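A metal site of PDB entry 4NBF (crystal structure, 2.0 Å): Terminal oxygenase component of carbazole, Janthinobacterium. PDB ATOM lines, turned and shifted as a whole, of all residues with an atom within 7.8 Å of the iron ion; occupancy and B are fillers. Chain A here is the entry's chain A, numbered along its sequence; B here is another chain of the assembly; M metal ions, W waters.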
ATOM      1  N   ASN A 177      30.821   1.522   2.009  1.00  0.00           N
ATOM      2  CA  ASN A 177      29.428   1.837   1.690  1.00  0.00           C
ATOM      3  C   ASN A 177      29.391   3.038   0.733  1.00  0.00           C
ATOM      4  O   ASN A 177      28.640   3.035  -0.242  1.00  0.00           O
ATOM      5  CB  ASN A 177      28.629   2.198   2.936  1.00  0.00           C
ATOM      6  CG  ASN A 177      27.220   2.680   2.605  1.00  0.00           C
ATOM      7  OD1 ASN A 177      26.352   1.883   2.277  1.00  0.00           O
ATOM      8  ND2 ASN A 177      27.008   3.988   2.668  1.00  0.00           N
ATOM      9  N   GLY A 178      30.194   4.060   1.025  1.00  0.00           N
ATOM     10  CA  GLY A 178      30.197   5.245   0.193  1.00  0.00           C
ATOM     11  C   GLY A 178      30.658   5.053  -1.244  1.00  0.00           C
ATOM     12  O   GLY A 178      30.152   5.707  -2.150  1.00  0.00           O
ATOM     13  N   PHE A 179      31.614   4.147  -1.449  1.00  0.00           N
ATOM     14  CA  PHE A 179      32.158   3.882  -2.782  1.00  0.00           C
ATOM     15  C   PHE A 179      31.437   2.707  -3.465  1.00  0.00           C
ATOM     16  O   PHE A 179      31.726   2.354  -4.603  1.00  0.00           O
ATOM     17  CB  PHE A 179      33.668   3.595  -2.665  1.00  0.00           C
ATOM     18  CG  PHE A 179      34.406   3.588  -3.987  1.00  0.00           C
ATOM     19  CD1 PHE A 179      34.346   4.682  -4.838  1.00  0.00           C
ATOM     20  CD2 PHE A 179      35.161   2.489  -4.365  1.00  0.00           C
ATOM     21  CE1 PHE A 179      35.033   4.690  -6.056  1.00  0.00           C
ATOM     22  CE2 PHE A 179      35.865   2.484  -5.571  1.00  0.00           C
ATOM     23  CZ  PHE A 179      35.791   3.580  -6.417  1.00  0.00           C
ATOM     24  N   ASP A 180      30.492   2.106  -2.741  1.00  0.00           N
ATOM     25  CA  ASP A 180      29.729   0.954  -3.231  1.00  0.00           C
ATOM     26  C   ASP A 180      28.769   1.387  -4.342  1.00  0.00           C
ATOM     27  O   ASP A 180      27.785   2.074  -4.087  1.00  0.00           O
ATOM     28  CB  ASP A 180      28.928   0.382  -2.052  1.00  0.00           C
ATOM     29  CG  ASP A 180      28.261  -0.947  -2.362  1.00  0.00           C
ATOM     30  OD1 ASP A 180      27.798  -1.129  -3.502  1.00  0.00           O
ATOM     31  OD2 ASP A 180      28.189  -1.793  -1.447  1.00  0.00           O
ATOM     32  N   HIS A 183      25.005   0.415  -3.745  1.00  0.00           N
ATOM     33  CA  HIS A 183      24.320   0.844  -2.519  1.00  0.00           C
ATOM     34  C   HIS A 183      23.332   1.969  -2.793  1.00  0.00           C
ATOM     35  O   HIS A 183      22.562   2.364  -1.916  1.00  0.00           O
ATOM     36  CB  HIS A 183      25.340   1.269  -1.436  1.00  0.00           C
ATOM     37  CG  HIS A 183      25.663   2.735  -1.443  1.00  0.00           C
ATOM     38  ND1 HIS A 183      26.504   3.313  -2.363  1.00  0.00           N
ATOM     39  CD2 HIS A 183      25.246   3.730  -0.630  1.00  0.00           C
ATOM     40  CE1 HIS A 183      26.583   4.613  -2.119  1.00  0.00           C
ATOM     41  NE2 HIS A 183      25.835   4.889  -1.069  1.00  0.00           N
ATOM     42  N   ILE A 184      23.361   2.474  -4.021  1.00  0.00           N
ATOM     43  CA  ILE A 184      22.469   3.529  -4.457  1.00  0.00           C
ATOM     44  C   ILE A 184      21.013   3.090  -4.213  1.00  0.00           C
ATOM     45  O   ILE A 184      20.113   3.924  -4.089  1.00  0.00           O
ATOM     46  CB  ILE A 184      22.690   3.821  -5.969  1.00  0.00           C
ATOM     47  CG1 ILE A 184      21.853   5.013  -6.416  1.00  0.00           C
ATOM     48  CG2 ILE A 184      22.308   2.602  -6.791  1.00  0.00           C
ATOM     49  CD1 ILE A 184      22.156   5.459  -7.850  1.00  0.00           C
ATOM     50  N   TYR A 185      20.806   1.784  -4.144  1.00  0.00           N
ATOM     51  CA  TYR A 185      19.473   1.236  -3.900  1.00  0.00           C
ATOM     52  C   TYR A 185      18.860   1.752  -2.586  1.00  0.00           C
ATOM     53  O   TYR A 185      17.659   1.993  -2.514  1.00  0.00           O
ATOM     54  CB  TYR A 185      19.541  -0.295  -3.853  1.00  0.00           C
ATOM     55  CG  TYR A 185      18.197  -1.004  -3.695  1.00  0.00           C
ATOM     56  CD1 TYR A 185      17.314  -1.103  -4.773  1.00  0.00           C
ATOM     57  CD2 TYR A 185      17.825  -1.583  -2.485  1.00  0.00           C
ATOM     58  CE1 TYR A 185      16.086  -1.769  -4.638  1.00  0.00           C
ATOM     59  CE2 TYR A 185      16.608  -2.250  -2.341  1.00  0.00           C
ATOM     60  CZ  TYR A 185      15.741  -2.335  -3.426  1.00  0.00           C
ATOM     61  OH  TYR A 185      14.552  -3.012  -3.283  1.00  0.00           O
ATOM     62  N   ILE A 186      19.685   1.950  -1.555  1.00  0.00           N
ATOM     63  CA  ILE A 186      19.162   2.424  -0.263  1.00  0.00           C
ATOM     64  C   ILE A 186      18.660   3.860  -0.320  1.00  0.00           C
ATOM     65  O   ILE A 186      17.980   4.311   0.608  1.00  0.00           O
ATOM     66  CB  ILE A 186      20.213   2.338   0.877  1.00  0.00           C
ATOM     67  CG1 ILE A 186      21.268   3.439   0.693  1.00  0.00           C
ATOM     68  CG2 ILE A 186      20.858   0.961   0.890  1.00  0.00           C
ATOM     69  CD1 ILE A 186      22.319   3.469   1.809  1.00  0.00           C
ATOM     70  N   HIS A 187      18.985   4.570  -1.390  1.00  0.00           N
ATOM     71  CA  HIS A 187      18.583   5.961  -1.545  1.00  0.00           C
ATOM     72  C   HIS A 187      17.346   6.162  -2.415  1.00  0.00           C
ATOM     73  O   HIS A 187      16.946   7.301  -2.657  1.00  0.00           O
ATOM     74  CB  HIS A 187      19.736   6.769  -2.127  1.00  0.00           C
ATOM     75  CG  HIS A 187      20.935   6.836  -1.237  1.00  0.00           C
ATOM     76  ND1 HIS A 187      20.899   7.402   0.015  1.00  0.00           N
ATOM     77  CD2 HIS A 187      22.203   6.394  -1.413  1.00  0.00           C
ATOM     78  CE1 HIS A 187      22.094   7.318   0.571  1.00  0.00           C
ATOM     79  NE2 HIS A 187      22.906   6.702  -0.273  1.00  0.00           N
ATOM     80  N   LEU A 270      35.789  10.350   0.130  1.00  0.00           N
ATOM     81  CA  LEU A 270      35.033  10.164  -1.102  1.00  0.00           C
ATOM     82  C   LEU A 270      34.685  11.498  -1.762  1.00  0.00           C
ATOM     83  O   LEU A 270      34.361  12.468  -1.081  1.00  0.00           O
ATOM     84  CB  LEU A 270      33.738   9.422  -0.808  1.00  0.00           C
ATOM     85  CG  LEU A 270      32.857   8.986  -1.988  1.00  0.00           C
ATOM     86  CD1 LEU A 270      33.408   7.688  -2.589  1.00  0.00           C
ATOM     87  CD2 LEU A 270      31.435   8.766  -1.495  1.00  0.00           C
ATOM     88  N   PHE A 275      27.303  16.807  -7.002  1.00  0.00           N
ATOM     89  CA  PHE A 275      26.315  16.372  -6.019  1.00  0.00           C
ATOM     90  C   PHE A 275      26.244  17.406  -4.899  1.00  0.00           C
ATOM     91  O   PHE A 275      27.266  17.979  -4.505  1.00  0.00           O
ATOM     92  CB  PHE A 275      26.718  15.009  -5.426  1.00  0.00           C
ATOM     93  CG  PHE A 275      25.601  14.305  -4.715  1.00  0.00           C
ATOM     94  CD1 PHE A 275      24.570  13.700  -5.440  1.00  0.00           C
ATOM     95  CD2 PHE A 275      25.561  14.257  -3.331  1.00  0.00           C
ATOM     96  CE1 PHE A 275      23.525  13.065  -4.786  1.00  0.00           C
ATOM     97  CE2 PHE A 275      24.513  13.625  -2.663  1.00  0.00           C
ATOM     98  CZ  PHE A 275      23.491  13.024  -3.387  1.00  0.00           C
ATOM     99  N   GLU A 284      33.469  13.777   1.380  1.00  0.00           N
ATOM    100  CA  GLU A 284      33.226  13.271   2.739  1.00  0.00           C
ATOM    101  C   GLU A 284      34.302  12.310   3.229  1.00  0.00           C
ATOM    102  O   GLU A 284      34.683  11.363   2.526  1.00  0.00           O
ATOM    103  CB  GLU A 284      31.842  12.609   2.839  1.00  0.00           C
ATOM    104  CG  GLU A 284      31.548  11.549   1.785  1.00  0.00           C
ATOM    105  CD  GLU A 284      30.217  10.847   2.016  1.00  0.00           C
ATOM    106  OE1 GLU A 284      29.214  11.546   2.294  1.00  0.00           O
ATOM    107  OE2 GLU A 284      30.156   9.592   1.928  1.00  0.00           O
ATOM    108  N   TYR A 286      35.807   9.700   6.373  1.00  0.00           N
ATOM    109  CA  TYR A 286      35.358   8.737   7.372  1.00  0.00           C
ATOM    110  C   TYR A 286      36.643   8.582   8.200  1.00  0.00           C
ATOM    111  O   TYR A 286      37.479   7.727   7.909  1.00  0.00           O
ATOM    112  CB  TYR A 286      34.977   7.420   6.717  1.00  0.00           C
ATOM    113  CG  TYR A 286      34.192   7.587   5.436  1.00  0.00           C
ATOM    114  CD1 TYR A 286      32.828   7.891   5.464  1.00  0.00           C
ATOM    115  CD2 TYR A 286      34.818   7.474   4.204  1.00  0.00           C
ATOM    116  CE1 TYR A 286      32.109   8.064   4.280  1.00  0.00           C
ATOM    117  CE2 TYR A 286      34.110   7.649   3.007  1.00  0.00           C
ATOM    118  CZ  TYR A 286      32.759   7.948   3.053  1.00  0.00           C
ATOM    119  OH  TYR A 286      32.060   8.125   1.879  1.00  0.00           O
ATOM    120  N   TYR A 296      32.232  11.320  10.724  1.00  0.00           N
ATOM    121  CA  TYR A 296      31.670  11.348   9.379  1.00  0.00           C
ATOM    122  C   TYR A 296      31.735  12.848   9.055  1.00  0.00           C
ATOM    123  O   TYR A 296      30.847  13.618   9.400  1.00  0.00           O
ATOM    124  CB  TYR A 296      30.220  10.829   9.403  1.00  0.00           C
ATOM    125  CG  TYR A 296      29.518  10.845   8.057  1.00  0.00           C
ATOM    126  CD1 TYR A 296      30.233  10.728   6.862  1.00  0.00           C
ATOM    127  CD2 TYR A 296      28.134  10.964   7.986  1.00  0.00           C
ATOM    128  CE1 TYR A 296      29.579  10.740   5.612  1.00  0.00           C
ATOM    129  CE2 TYR A 296      27.471  10.969   6.756  1.00  0.00           C
ATOM    130  CZ  TYR A 296      28.202  10.863   5.577  1.00  0.00           C
ATOM    131  OH  TYR A 296      27.538  10.911   4.363  1.00  0.00           O
ATOM    132  N   PHE A 329      19.715  12.826   2.645  1.00  0.00           N
ATOM    133  CA  PHE A 329      20.219  11.784   1.760  1.00  0.00           C
ATOM    134  C   PHE A 329      21.177  10.852   2.486  1.00  0.00           C
ATOM    135  O   PHE A 329      20.970   9.641   2.519  1.00  0.00           O
ATOM    136  CB  PHE A 329      20.935  12.415   0.565  1.00  0.00           C
ATOM    137  CG  PHE A 329      21.324  11.435  -0.509  1.00  0.00           C
ATOM    138  CD1 PHE A 329      20.415  11.061  -1.500  1.00  0.00           C
ATOM    139  CD2 PHE A 329      22.605  10.896  -0.546  1.00  0.00           C
ATOM    140  CE1 PHE A 329      20.778  10.186  -2.514  1.00  0.00           C
ATOM    141  CE2 PHE A 329      22.983  10.013  -1.556  1.00  0.00           C
ATOM    142  CZ  PHE A 329      22.064   9.659  -2.544  1.00  0.00           C
ATOM    143  N   ASN A 330      22.213  11.425   3.093  1.00  0.00           N
ATOM    144  CA  ASN A 330      23.231  10.626   3.781  1.00  0.00           C
ATOM    145  C   ASN A 330      22.821   9.928   5.082  1.00  0.00           C
ATOM    146  O   ASN A 330      23.530   9.029   5.536  1.00  0.00           O
ATOM    147  CB  ASN A 330      24.480  11.491   4.019  1.00  0.00           C
ATOM    148  CG  ASN A 330      25.140  11.919   2.721  1.00  0.00           C
ATOM    149  OD1 ASN A 330      25.495  13.088   2.546  1.00  0.00           O
ATOM    150  ND2 ASN A 330      25.314  10.979   1.794  1.00  0.00           N
ATOM    151  N   ASN A 331      21.711  10.312   5.692  1.00  0.00           N
ATOM    152  CA  ASN A 331      21.337   9.623   6.917  1.00  0.00           C
ATOM    153  C   ASN A 331      21.144   8.128   6.661  1.00  0.00           C
ATOM    154  O   ASN A 331      21.427   7.301   7.533  1.00  0.00           O
ATOM    155  CB  ASN A 331      20.085  10.234   7.557  1.00  0.00           C
ATOM    156  CG  ASN A 331      20.402  11.442   8.399  1.00  0.00           C
ATOM    157  OD1 ASN A 331      21.570  11.700   8.719  1.00  0.00           O
ATOM    158  ND2 ASN A 331      19.380  12.203   8.780  1.00  0.00           N
ATOM    159  N   ASP A 332      20.691   7.761   5.463  1.00  0.00           N
ATOM    160  CA  ASP A 332      20.530   6.344   5.165  1.00  0.00           C
ATOM    161  C   ASP A 332      21.886   5.646   5.084  1.00  0.00           C
ATOM    162  O   ASP A 332      21.998   4.451   5.343  1.00  0.00           O
ATOM    163  CB  ASP A 332      19.759   6.135   3.861  1.00  0.00           C
ATOM    164  CG  ASP A 332      18.272   6.415   4.010  1.00  0.00           C
ATOM    165  OD1 ASP A 332      17.696   5.963   5.021  1.00  0.00           O
ATOM    166  OD2 ASP A 332      17.688   7.060   3.128  1.00  0.00           O
ATOM    167  N   ASP A 333      22.933   6.399   4.732  1.00  0.00           N
ATOM    168  CA  ASP A 333      24.264   5.816   4.645  1.00  0.00           C
ATOM    169  C   ASP A 333      24.753   5.459   6.041  1.00  0.00           C
ATOM    170  O   ASP A 333      25.490   4.488   6.228  1.00  0.00           O
ATOM    171  CB  ASP A 333      25.241   6.805   4.000  1.00  0.00           C
ATOM    172  CG  ASP A 333      24.972   6.987   2.529  1.00  0.00           C
ATOM    173  OD1 ASP A 333      24.923   5.958   1.823  1.00  0.00           O
ATOM    174  OD2 ASP A 333      24.800   8.135   2.085  1.00  0.00           O
ATOM    175  N   ILE A 334      24.333   6.251   7.028  1.00  0.00           N
ATOM    176  CA  ILE A 334      24.739   6.016   8.399  1.00  0.00           C
ATOM    177  C   ILE A 334      24.204   4.689   8.937  1.00  0.00           C
ATOM    178  O   ILE A 334      24.985   3.880   9.456  1.00  0.00           O
ATOM    179  CB  ILE A 334      24.286   7.171   9.320  1.00  0.00           C
ATOM    180  CG1 ILE A 334      25.122   8.414   9.034  1.00  0.00           C
ATOM    181  CG2 ILE A 334      24.423   6.762  10.787  1.00  0.00           C
ATOM    182  CD1 ILE A 334      24.608   9.695   9.688  1.00  0.00           C
ATOM    183  N   ALA A 336      23.117   2.127   7.227  1.00  0.00           N
ATOM    184  CA  ALA A 336      23.528   0.995   6.390  1.00  0.00           C
ATOM    185  C   ALA A 336      24.918   0.583   6.889  1.00  0.00           C
ATOM    186  O   ALA A 336      25.239  -0.597   7.015  1.00  0.00           O
ATOM    187  CB  ALA A 336      23.601   1.411   4.929  1.00  0.00           C
ATOM    188  N   ARG A 337      25.713   1.604   7.158  1.00  0.00           N
ATOM    189  CA  ARG A 337      27.065   1.484   7.681  1.00  0.00           C
ATOM    190  C   ARG A 337      27.011   0.663   8.980  1.00  0.00           C
ATOM    191  O   ARG A 337      27.741  -0.315   9.153  1.00  0.00           O
ATOM    192  CB  ARG A 337      27.547   2.912   7.974  1.00  0.00           C
ATOM    193  CG  ARG A 337      29.002   3.145   8.130  1.00  0.00           C
ATOM    194  CD  ARG A 337      29.227   4.640   8.283  1.00  0.00           C
ATOM    195  NE  ARG A 337      28.691   5.395   7.147  1.00  0.00           N
ATOM    196  CZ  ARG A 337      28.775   6.710   7.027  1.00  0.00           C
ATOM    197  NH1 ARG A 337      29.377   7.429   7.967  1.00  0.00           N
ATOM    198  NH2 ARG A 337      28.267   7.328   5.967  1.00  0.00           N
ATOM    199  N   TYR B  92      19.676  -3.555   1.305  1.00  0.00           N
ATOM    200  CA  TYR B  92      20.971  -2.975   0.934  1.00  0.00           C
ATOM    201  C   TYR B  92      21.280  -2.968  -0.573  1.00  0.00           C
ATOM    202  O   TYR B  92      21.331  -1.894  -1.185  1.00  0.00           O
ATOM    203  CB  TYR B  92      22.088  -3.698   1.707  1.00  0.00           C
ATOM    204  CG  TYR B  92      23.318  -2.851   2.010  1.00  0.00           C
ATOM    205  CD1 TYR B  92      23.503  -1.603   1.417  1.00  0.00           C
ATOM    206  CD2 TYR B  92      24.307  -3.337   2.865  1.00  0.00           C
ATOM    207  CE1 TYR B  92      24.651  -0.854   1.677  1.00  0.00           C
ATOM    208  CE2 TYR B  92      25.461  -2.601   3.128  1.00  0.00           C
ATOM    209  CZ  TYR B  92      25.628  -1.361   2.533  1.00  0.00           C
ATOM    210  OH  TYR B  92      26.771  -0.643   2.775  1.00  0.00           O
HETATM  211 FE    FE M   1      24.993   6.460  -0.065  1.00  0.00          FE
HETATM  212  O   HOH W   1      26.541   7.734  -0.190  1.00  0.00           O
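The side-chain amide nitrogen (ND2) of Asn 330 lies within hydrogen-bond range of the side-chain carboxylate (OD2) of Asp 333 (2.9 Å).
The backbone carbonyl oxygen (O) of Asp 333 lies close to the guanidinium group (NE) of Arg 337 (3.5 Å).
ND1 of His 187 sits close to O of Phe 329, 3.4 Å away.
The side-chain carboxylate of Asp 333 sits close to the side-chain amide nitrogen of Asn 177 (3.0 Å).
A ring nitrogen (ND1) of His 183 is in hydrogen-bond range of the backbone carbonyl oxygen (O) of Asp 180, 2.5 Å away.
A ring nitrogen (ND1) of His 183 sits at hydrogen-bond distance from the backbone carbonyl oxygen of Asn 177 (3.0 Å).
Within 4 Å of the iron ion: His 183, His 187 and Asp 333.
OD1 of Asp 333 binds the iron ion (2.0 Å).
Water W1 binds the iron ion (2.0 Å).
NE2 of His 183 is bound to the iron ion, at 2.0 Å.
The iron ion is bound by NE2 of His 187 (2.1 Å).
Slightly farther from the iron ion lies OD2 of Asp 333 (2.7 Å).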
